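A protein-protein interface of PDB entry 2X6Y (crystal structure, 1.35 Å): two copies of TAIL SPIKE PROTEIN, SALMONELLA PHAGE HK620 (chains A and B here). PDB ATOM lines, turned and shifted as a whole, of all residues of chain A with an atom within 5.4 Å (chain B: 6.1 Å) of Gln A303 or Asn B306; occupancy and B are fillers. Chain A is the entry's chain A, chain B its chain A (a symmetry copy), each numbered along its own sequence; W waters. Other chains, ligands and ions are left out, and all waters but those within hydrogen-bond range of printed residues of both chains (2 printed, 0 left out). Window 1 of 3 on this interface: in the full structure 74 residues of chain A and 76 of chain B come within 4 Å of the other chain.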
ATOM      1  N   LEU A 264      29.997  24.301  29.023  1.00  0.00           N
ATOM      2  CA  LEU A 264      29.660  23.081  28.291  1.00  0.00           C
ATOM      3  C   LEU A 264      30.932  22.584  27.620  1.00  0.00           C
ATOM      4  O   LEU A 264      31.467  23.248  26.732  1.00  0.00           O
ATOM      5  CB  LEU A 264      28.598  23.364  27.230  1.00  0.00           C
ATOM      6  CG  LEU A 264      27.261  23.951  27.721  1.00  0.00           C
ATOM      7  CD1 LEU A 264      26.283  24.111  26.571  1.00  0.00           C
ATOM      8  CD2 LEU A 264      26.678  23.082  28.853  1.00  0.00           C
ATOM      9  N   THR A 269      25.429  18.624  24.755  1.00  0.00           N
ATOM     10  CA  THR A 269      25.115  19.317  25.975  1.00  0.00           C
ATOM     11  C   THR A 269      24.397  20.626  25.688  1.00  0.00           C
ATOM     12  O   THR A 269      24.465  21.184  24.587  1.00  0.00           O
ATOM     13  CB  THR A 269      26.365  19.560  26.848  1.00  0.00           C
ATOM     14  OG1 THR A 269      27.328  20.341  26.125  1.00  0.00           O
ATOM     15  CG2 THR A 269      26.977  18.236  27.325  1.00  0.00           C
ATOM     16  N   PHE A 270      23.674  21.101  26.697  1.00  0.00           N
ATOM     17  CA  PHE A 270      22.786  22.225  26.524  1.00  0.00           C
ATOM     18  C   PHE A 270      22.685  23.114  27.737  1.00  0.00           C
ATOM     19  O   PHE A 270      22.886  22.691  28.867  1.00  0.00           O
ATOM     20  CB  PHE A 270      21.379  21.766  26.106  1.00  0.00           C
ATOM     21  CG  PHE A 270      20.687  20.889  27.108  1.00  0.00           C
ATOM     22  CD1 PHE A 270      19.980  21.430  28.169  1.00  0.00           C
ATOM     23  CD2 PHE A 270      20.742  19.520  26.994  1.00  0.00           C
ATOM     24  CE1 PHE A 270      19.326  20.612  29.094  1.00  0.00           C
ATOM     25  CE2 PHE A 270      20.104  18.711  27.919  1.00  0.00           C
ATOM     26  CZ  PHE A 270      19.374  19.257  28.952  1.00  0.00           C
ATOM     27  N   TYR A 271      22.326  24.356  27.452  1.00  0.00           N
ATOM     28  CA  TYR A 271      22.040  25.366  28.458  1.00  0.00           C
ATOM     29  C   TYR A 271      20.854  26.185  27.959  1.00  0.00           C
ATOM     30  O   TYR A 271      20.991  26.935  26.993  1.00  0.00           O
ATOM     31  CB  TYR A 271      23.271  26.249  28.656  1.00  0.00           C
ATOM     32  CG  TYR A 271      23.123  27.370  29.656  1.00  0.00           C
ATOM     33  CD1 TYR A 271      22.233  27.288  30.738  1.00  0.00           C
ATOM     34  CD2 TYR A 271      23.915  28.503  29.558  1.00  0.00           C
ATOM     35  CE1 TYR A 271      22.139  28.331  31.667  1.00  0.00           C
ATOM     36  CE2 TYR A 271      23.804  29.531  30.475  1.00  0.00           C
ATOM     37  CZ  TYR A 271      22.923  29.438  31.525  1.00  0.00           C
ATOM     38  OH  TYR A 271      22.865  30.445  32.468  1.00  0.00           O
ATOM     39  N   ARG A 272      19.694  26.014  28.601  1.00  0.00           N
ATOM     40  CA  ARG A 272      18.458  26.585  28.097  1.00  0.00           C
ATOM     41  C   ARG A 272      17.607  27.222  29.187  1.00  0.00           C
ATOM     42  O   ARG A 272      17.626  26.794  30.355  1.00  0.00           O
ATOM     43  CB  ARG A 272      17.596  25.480  27.453  1.00  0.00           C
ATOM     44  CG  ARG A 272      18.230  24.704  26.297  1.00  0.00           C
ATOM     45  CD  ARG A 272      17.162  23.907  25.555  1.00  0.00           C
ATOM     46  NE  ARG A 272      16.612  22.858  26.413  1.00  0.00           N
ATOM     47  CZ  ARG A 272      16.802  21.540  26.259  1.00  0.00           C
ATOM     48  NH1 ARG A 272      17.538  21.052  25.267  1.00  0.00           N
ATOM     49  NH2 ARG A 272      16.239  20.698  27.117  1.00  0.00           N
ATOM     50  N   ASN A 301      27.094  19.278  18.821  1.00  0.00           N
ATOM     51  CA  ASN A 301      25.713  19.331  19.322  1.00  0.00           C
ATOM     52  C   ASN A 301      25.659  20.074  20.648  1.00  0.00           C
ATOM     53  O   ASN A 301      25.257  19.538  21.692  1.00  0.00           O
ATOM     54  CB  ASN A 301      25.089  17.934  19.443  1.00  0.00           C
ATOM     55  CG  ASN A 301      24.595  17.405  18.136  1.00  0.00           C
ATOM     56  OD1 ASN A 301      24.533  18.139  17.145  1.00  0.00           O
ATOM     57  ND2 ASN A 301      24.196  16.131  18.127  1.00  0.00           N
ATOM     58  N   MET A 302      26.081  21.329  20.584  1.00  0.00           N
ATOM     59  CA  MET A 302      26.145  22.212  21.736  1.00  0.00           C
ATOM     60  C   MET A 302      25.057  23.264  21.554  1.00  0.00           C
ATOM     61  O   MET A 302      25.021  23.942  20.547  1.00  0.00           O
ATOM     62  CB  MET A 302      27.525  22.895  21.837  1.00  0.00           C
ATOM     63  CG  MET A 302      28.731  22.002  21.583  1.00  0.00           C
ATOM     64  SD  MET A 302      28.959  20.696  22.830  1.00  0.00           S
ATOM     65  CE  MET A 302      29.675  21.714  24.170  1.00  0.00           C
ATOM     66  N   GLN A 303      24.192  23.415  22.552  1.00  0.00           N
ATOM     67  CA  GLN A 303      23.009  24.251  22.424  1.00  0.00           C
ATOM     68  C   GLN A 303      22.919  25.284  23.556  1.00  0.00           C
ATOM     69  O   GLN A 303      22.930  24.917  24.718  1.00  0.00           O
ATOM     70  CB  GLN A 303      21.784  23.337  22.429  1.00  0.00           C
ATOM     71  CG  GLN A 303      20.453  23.998  22.307  1.00  0.00           C
ATOM     72  CD  GLN A 303      19.351  22.961  22.425  1.00  0.00           C
ATOM     73  OE1 GLN A 303      19.267  22.269  23.423  1.00  0.00           O
ATOM     74  NE2 GLN A 303      18.541  22.826  21.402  1.00  0.00           N
ATOM     75  N   VAL A 304      22.847  26.571  23.202  1.00  0.00           N
ATOM     76  CA  VAL A 304      22.630  27.644  24.178  1.00  0.00           C
ATOM     77  C   VAL A 304      21.409  28.404  23.692  1.00  0.00           C
ATOM     78  O   VAL A 304      21.492  29.152  22.719  1.00  0.00           O
ATOM     79  CB  VAL A 304      23.857  28.585  24.311  1.00  0.00           C
ATOM     80  CG1 VAL A 304      23.582  29.657  25.346  1.00  0.00           C
ATOM     81  CG2 VAL A 304      25.091  27.806  24.745  1.00  0.00           C
ATOM     82  N   GLU A 305      20.280  28.205  24.365  1.00  0.00           N
ATOM     83  CA  GLU A 305      19.020  28.704  23.837  1.00  0.00           C
ATOM     84  C   GLU A 305      18.064  29.290  24.878  1.00  0.00           C
ATOM     85  O   GLU A 305      17.949  28.791  25.989  1.00  0.00           O
ATOM     86  CB  GLU A 305      18.295  27.567  23.086  1.00  0.00           C
ATOM     87  CG  GLU A 305      18.859  27.282  21.720  1.00  0.00           C
ATOM     88  CD  GLU A 305      18.137  26.192  20.945  1.00  0.00           C
ATOM     89  OE1 GLU A 305      17.423  25.385  21.574  1.00  0.00           O
ATOM     90  OE2 GLU A 305      18.328  26.122  19.706  1.00  0.00           O
ATOM     91  N   ASN A 306      17.410  30.381  24.488  1.00  0.00           N
ATOM     92  CA  ASN A 306      16.262  30.947  25.215  1.00  0.00           C
ATOM     93  C   ASN A 306      16.611  31.342  26.649  1.00  0.00           C
ATOM     94  O   ASN A 306      15.805  31.219  27.558  1.00  0.00           O
ATOM     95  CB  ASN A 306      15.077  29.966  25.240  1.00  0.00           C
ATOM     96  CG  ASN A 306      14.518  29.674  23.863  1.00  0.00           C
ATOM     97  OD1 ASN A 306      15.074  30.078  22.849  1.00  0.00           O
ATOM     98  ND2 ASN A 306      13.400  28.959  23.828  1.00  0.00           N
ATOM     99  N   ILE A 334      24.646  25.695  18.274  1.00  0.00           N
ATOM    100  CA  ILE A 334      23.553  26.626  18.018  1.00  0.00           C
ATOM    101  C   ILE A 334      23.345  27.528  19.230  1.00  0.00           C
ATOM    102  O   ILE A 334      23.229  27.046  20.367  1.00  0.00           O
ATOM    103  CB  ILE A 334      22.275  25.864  17.590  1.00  0.00           C
ATOM    104  CG1 ILE A 334      21.237  26.841  17.043  1.00  0.00           C
ATOM    105  CG2 ILE A 334      21.726  24.974  18.720  1.00  0.00           C
ATOM    106  CD1 ILE A 334      20.063  26.226  16.301  1.00  0.00           C
ATOM    107  N   SER A 336      20.693  30.461  20.108  1.00  0.00           N
ATOM    108  CA  SER A 336      19.460  31.016  19.577  1.00  0.00           C
ATOM    109  C   SER A 336      18.476  31.429  20.650  1.00  0.00           C
ATOM    110  O   SER A 336      18.381  30.812  21.692  1.00  0.00           O
ATOM    111  CB  SER A 336      18.792  29.999  18.654  1.00  0.00           C
ATOM    112  OG  SER A 336      18.380  28.859  19.373  1.00  0.00           O
ATOM    113  N   TYR B 271       6.931  18.618  20.379  1.00  0.00           N
ATOM    114  CA  TYR B 271       8.127  17.848  20.681  1.00  0.00           C
ATOM    115  C   TYR B 271       9.278  18.834  20.838  1.00  0.00           C
ATOM    116  O   TYR B 271       9.704  19.440  19.855  1.00  0.00           O
ATOM    117  CB  TYR B 271       8.398  16.865  19.543  1.00  0.00           C
ATOM    118  CG  TYR B 271       9.629  16.005  19.694  1.00  0.00           C
ATOM    119  CD1 TYR B 271      10.141  15.659  20.955  1.00  0.00           C
ATOM    120  CD2 TYR B 271      10.260  15.484  18.577  1.00  0.00           C
ATOM    121  CE1 TYR B 271      11.268  14.835  21.065  1.00  0.00           C
ATOM    122  CE2 TYR B 271      11.378  14.681  18.700  1.00  0.00           C
ATOM    123  CZ  TYR B 271      11.872  14.357  19.940  1.00  0.00           C
ATOM    124  OH  TYR B 271      12.953  13.504  20.051  1.00  0.00           O
ATOM    125  N   ARG B 272       9.753  19.010  22.075  1.00  0.00           N
ATOM    126  CA  ARG B 272      10.708  20.060  22.378  1.00  0.00           C
ATOM    127  C   ARG B 272      11.839  19.595  23.286  1.00  0.00           C
ATOM    128  O   ARG B 272      11.664  18.697  24.129  1.00  0.00           O
ATOM    129  CB  ARG B 272       9.999  21.217  23.112  1.00  0.00           C
ATOM    130  CG  ARG B 272       8.830  21.878  22.380  1.00  0.00           C
ATOM    131  CD  ARG B 272       8.465  23.193  23.060  1.00  0.00           C
ATOM    132  NE  ARG B 272       7.937  22.951  24.402  1.00  0.00           N
ATOM    133  CZ  ARG B 272       6.667  23.130  24.789  1.00  0.00           C
ATOM    134  NH1 ARG B 272       5.736  23.564  23.946  1.00  0.00           N
ATOM    135  NH2 ARG B 272       6.327  22.870  26.045  1.00  0.00           N
ATOM    136  N   GLY B 273      12.985  20.262  23.148  1.00  0.00           N
ATOM    137  CA  GLY B 273      14.050  20.178  24.151  1.00  0.00           C
ATOM    138  C   GLY B 273      14.618  18.804  24.415  1.00  0.00           C
ATOM    139  O   GLY B 273      15.134  18.541  25.504  1.00  0.00           O
ATOM    140  N   SER B 274      14.583  17.936  23.412  1.00  0.00           N
ATOM    141  CA  SER B 274      14.997  16.562  23.603  1.00  0.00           C
ATOM    142  C   SER B 274      16.264  16.273  22.816  1.00  0.00           C
ATOM    143  O   SER B 274      16.623  17.006  21.889  1.00  0.00           O
ATOM    144  CB  SER B 274      13.850  15.632  23.210  1.00  0.00           C
ATOM    145  OG  SER B 274      12.712  15.854  24.027  1.00  0.00           O
ATOM    146  N   VAL B 304       7.889  21.464  16.606  1.00  0.00           N
ATOM    147  CA  VAL B 304       9.104  20.670  16.816  1.00  0.00           C
ATOM    148  C   VAL B 304      10.222  21.674  17.031  1.00  0.00           C
ATOM    149  O   VAL B 304      10.669  22.316  16.083  1.00  0.00           O
ATOM    150  CB  VAL B 304       9.417  19.734  15.617  1.00  0.00           C
ATOM    151  CG1 VAL B 304      10.665  18.926  15.899  1.00  0.00           C
ATOM    152  CG2 VAL B 304       8.267  18.769  15.372  1.00  0.00           C
ATOM    153  N   GLU B 305      10.663  21.810  18.279  1.00  0.00           N
ATOM    154  CA  GLU B 305      11.562  22.903  18.617  1.00  0.00           C
ATOM    155  C   GLU B 305      12.685  22.543  19.592  1.00  0.00           C
ATOM    156  O   GLU B 305      12.496  21.779  20.527  1.00  0.00           O
ATOM    157  CB  GLU B 305      10.746  24.070  19.211  1.00  0.00           C
ATOM    158  CG  GLU B 305      10.001  24.879  18.183  1.00  0.00           C
ATOM    159  CD  GLU B 305       9.220  26.058  18.741  1.00  0.00           C
ATOM    160  OE1 GLU B 305       8.937  26.065  19.956  1.00  0.00           O
ATOM    161  OE2 GLU B 305       8.853  26.954  17.943  1.00  0.00           O
ATOM    162  N   ASN B 306      13.862  23.100  19.321  1.00  0.00           N
ATOM    163  CA  ASN B 306      14.996  23.109  20.260  1.00  0.00           C
ATOM    164  C   ASN B 306      15.447  21.702  20.649  1.00  0.00           C
ATOM    165  O   ASN B 306      15.857  21.452  21.773  1.00  0.00           O
ATOM    166  CB  ASN B 306      14.657  23.898  21.538  1.00  0.00           C
ATOM    167  CG  ASN B 306      14.400  25.367  21.278  1.00  0.00           C
ATOM    168  OD1 ASN B 306      14.329  25.812  20.139  1.00  0.00           O
ATOM    169  ND2 ASN B 306      14.256  26.132  22.354  1.00  0.00           N
ATOM    170  N   ASN B 307      15.382  20.791  19.688  1.00  0.00           N
ATOM    171  CA  ASN B 307      15.899  19.444  19.871  1.00  0.00           C
ATOM    172  C   ASN B 307      17.313  19.318  19.307  1.00  0.00           C
ATOM    173  O   ASN B 307      17.743  20.102  18.460  1.00  0.00           O
ATOM    174  CB  ASN B 307      14.989  18.440  19.187  1.00  0.00           C
ATOM    175  CG  ASN B 307      13.571  18.487  19.713  1.00  0.00           C
ATOM    176  OD1 ASN B 307      13.324  18.174  20.880  1.00  0.00           O
ATOM    177  ND2 ASN B 307      12.618  18.875  18.852  1.00  0.00           N
ATOM    178  N   ILE B 308      17.987  18.277  19.765  1.00  0.00           N
ATOM    179  CA  ILE B 308      19.350  17.955  19.399  1.00  0.00           C
ATOM    180  C   ILE B 308      19.298  16.512  18.867  1.00  0.00           C
ATOM    181  O   ILE B 308      18.803  15.638  19.562  1.00  0.00           O
ATOM    182  CB  ILE B 308      20.278  17.977  20.633  1.00  0.00           C
ATOM    183  CG1 ILE B 308      20.379  19.376  21.244  1.00  0.00           C
ATOM    184  CG2 ILE B 308      21.660  17.489  20.259  1.00  0.00           C
ATOM    185  CD1 ILE B 308      21.102  19.401  22.606  1.00  0.00           C
ATOM    186  N   SER B 336      11.704  24.719  14.558  1.00  0.00           N
ATOM    187  CA  SER B 336      12.639  25.791  14.851  1.00  0.00           C
ATOM    188  C   SER B 336      13.627  25.445  15.943  1.00  0.00           C
ATOM    189  O   SER B 336      13.313  24.737  16.879  1.00  0.00           O
ATOM    190  CB  SER B 336      11.871  27.048  15.254  1.00  0.00           C
ATOM    191  OG  SER B 336      11.179  26.850  16.465  1.00  0.00           O
ATOM    192  N   GLY B 337      14.834  25.987  15.832  1.00  0.00           N
ATOM    193  CA  GLY B 337      15.833  25.863  16.894  1.00  0.00           C
ATOM    194  C   GLY B 337      16.493  24.508  17.033  1.00  0.00           C
ATOM    195  O   GLY B 337      17.165  24.256  18.019  1.00  0.00           O
ATOM    196  N   ASN B 338      16.259  23.603  16.083  1.00  0.00           N
ATOM    197  CA  ASN B 338      16.814  22.259  16.173  1.00  0.00           C
ATOM    198  C   ASN B 338      18.212  22.231  15.600  1.00  0.00           C
ATOM    199  O   ASN B 338      18.505  22.917  14.628  1.00  0.00           O
ATOM    200  CB  ASN B 338      15.924  21.260  15.402  1.00  0.00           C
ATOM    201  CG  ASN B 338      14.495  21.261  15.911  1.00  0.00           C
ATOM    202  OD1 ASN B 338      14.223  20.715  16.967  1.00  0.00           O
ATOM    203  ND2 ASN B 338      13.574  21.906  15.164  1.00  0.00           N
ATOM    204  N   ILE B 339      19.054  21.401  16.197  1.00  0.00           N
ATOM    205  CA  ILE B 339      20.379  21.151  15.665  1.00  0.00           C
ATOM    206  C   ILE B 339      20.489  19.662  15.391  1.00  0.00           C
ATOM    207  O   ILE B 339      20.341  18.849  16.302  1.00  0.00           O
ATOM    208  CB  ILE B 339      21.507  21.697  16.579  1.00  0.00           C
ATOM    209  CG1 ILE B 339      22.867  21.374  15.950  1.00  0.00           C
ATOM    210  CG2 ILE B 339      21.380  21.214  17.999  1.00  0.00           C
ATOM    211  CD1 ILE B 339      23.994  22.259  16.457  1.00  0.00           C
ATOM    212  N   ASN B 379      17.060  26.631  12.239  1.00  0.00           N
ATOM    213  CA  ASN B 379      17.625  25.293  12.475  1.00  0.00           C
ATOM    214  C   ASN B 379      18.970  25.181  11.816  1.00  0.00           C
ATOM    215  O   ASN B 379      19.276  25.904  10.865  1.00  0.00           O
ATOM    216  CB  ASN B 379      16.745  24.216  11.848  1.00  0.00           C
ATOM    217  CG  ASN B 379      15.317  24.282  12.320  1.00  0.00           C
ATOM    218  OD1 ASN B 379      14.996  23.819  13.419  1.00  0.00           O
ATOM    219  ND2 ASN B 379      14.435  24.845  11.491  1.00  0.00           N
HETATM  220  O   HOH W   1      17.853  17.702  25.473  1.00  0.00           O
HETATM  221  O   HOH W   2      15.756  28.901  20.268  1.00  0.00           O
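Of the printed residues of chain B, Glu A305 touches Asn B306 and Gly B337. Of the printed residues of chain B, Asn A306 touches Asn B306. Tyr B271 touches none of the printed residues of chain A. Ser B274 touches none of the printed residues of chain A. Of the printed residues of chain A, Asn B306 touches Arg A272 (3.9 Å), Gln A303 (3.0 Å), Glu A305 (3.0 Å) and Asn A306 (3.3 Å). Of the printed residues of chain A, Gly B337 touches Gln A303 (3.9 Å), Glu A305 (2.8 Å) and Ile A334 (3.9 Å). Of the printed residues of chain A, Ile B339 touches Asn A301 and Ile A334. The nearest printed residue of chain B that does not touch Gln A303 is Asn B307 (4.1 Å). The nearest printed residue of chain A that does not touch Asn B306 is Ser A336 (5.1 Å).
Arg A272 touches Asn B306, but with the chains exchanged Asn A306 does not touch Arg B272 (7.6 Å). Glu A305 touches Asn B306, but with the chains exchanged Asn A306 does not touch Glu B305 (6.6 Å). Asn B306 touches its own counterpart, Asn A306. Positions printed for both chains: 271, 272, 304, 305, 306 and 336. Of the 12 pairs that touch across the chains among the printed residues, 1 has its exchanged pair printed and touching as well.
Among the printed residues, merely in contact across the chains: Gln A303 with Ile B308 (3.5 Å), Asn A301 with Ile B308 (3.6 Å), Asn A301 with Ile B339 (3.8 Å), Ile A334 with Ile B339 (3.8 Å), Arg A272 with Asn B306 (3.9 Å), Ile A334 with Gly B337 (3.9 Å) and Gln A303 with Gly B337 (3.9 Å).
Water W2 lies within hydrogen-bond range of OG of Ser A336, OD1 of Asn A306 and OD1 of Asn B306. Water W1 lies within hydrogen-bond range of O of Gly B273 (2.8 Å) and NH1 of Arg A272 (3.4 Å).
The side-chain carboxylate (OE1) of Glu A305 lies close to the side-chain amide nitrogen (ND2) of Asn B306, 3.3 Å away. The side-chain amide nitrogen (ND2) of Asn A306 lies close to the side-chain amide nitrogen (ND2) of Asn B306, at 3.3 Å. The side-chain amide nitrogen (NE2) of Gln A303 sits at hydrogen-bond distance from the backbone carbonyl oxygen (O) of Asn B306, at 3.0 Å. The side-chain carboxylate of Glu A305 sits close to the backbone carbonyl oxygen of Gly B337 (2.8 Å). O of Gly B273 sits at hydrogen-bond distance from NH2 of Arg A272 (2.9 Å).
The backbone NH of Val A304 sits at hydrogen-bond distance from the backbone carbonyl oxygen of Ile A334, 2.9 Å away. O of Ser A336 lies within hydrogen-bond range of N of Asn A306, 3.0 Å away. OE2 of Glu A305 is in hydrogen-bond range of OG of Ser A336 (2.8 Å). The backbone carbonyl oxygen (O) of Met A302 is in hydrogen-bond range of the backbone NH (N) of Ile A334, at 2.9 Å. The backbone NH of Gly B273 sits at hydrogen-bond distance from the backbone carbonyl oxygen of Glu B305 (3.1 Å). The backbone NH of Asn B306 sits at hydrogen-bond distance from the side-chain amide oxygen of Asn B338, at 3.4 Å.
Hydrophobic or aromatic side chains of chain A within 4 Å of the printed part of chain B: Ile A334. Hydrophobic or aromatic side chains of chain B that line the printed part of chain A: Ile B308 and Ile B339. Among the printed residues, 12 pairs touch across the chains.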
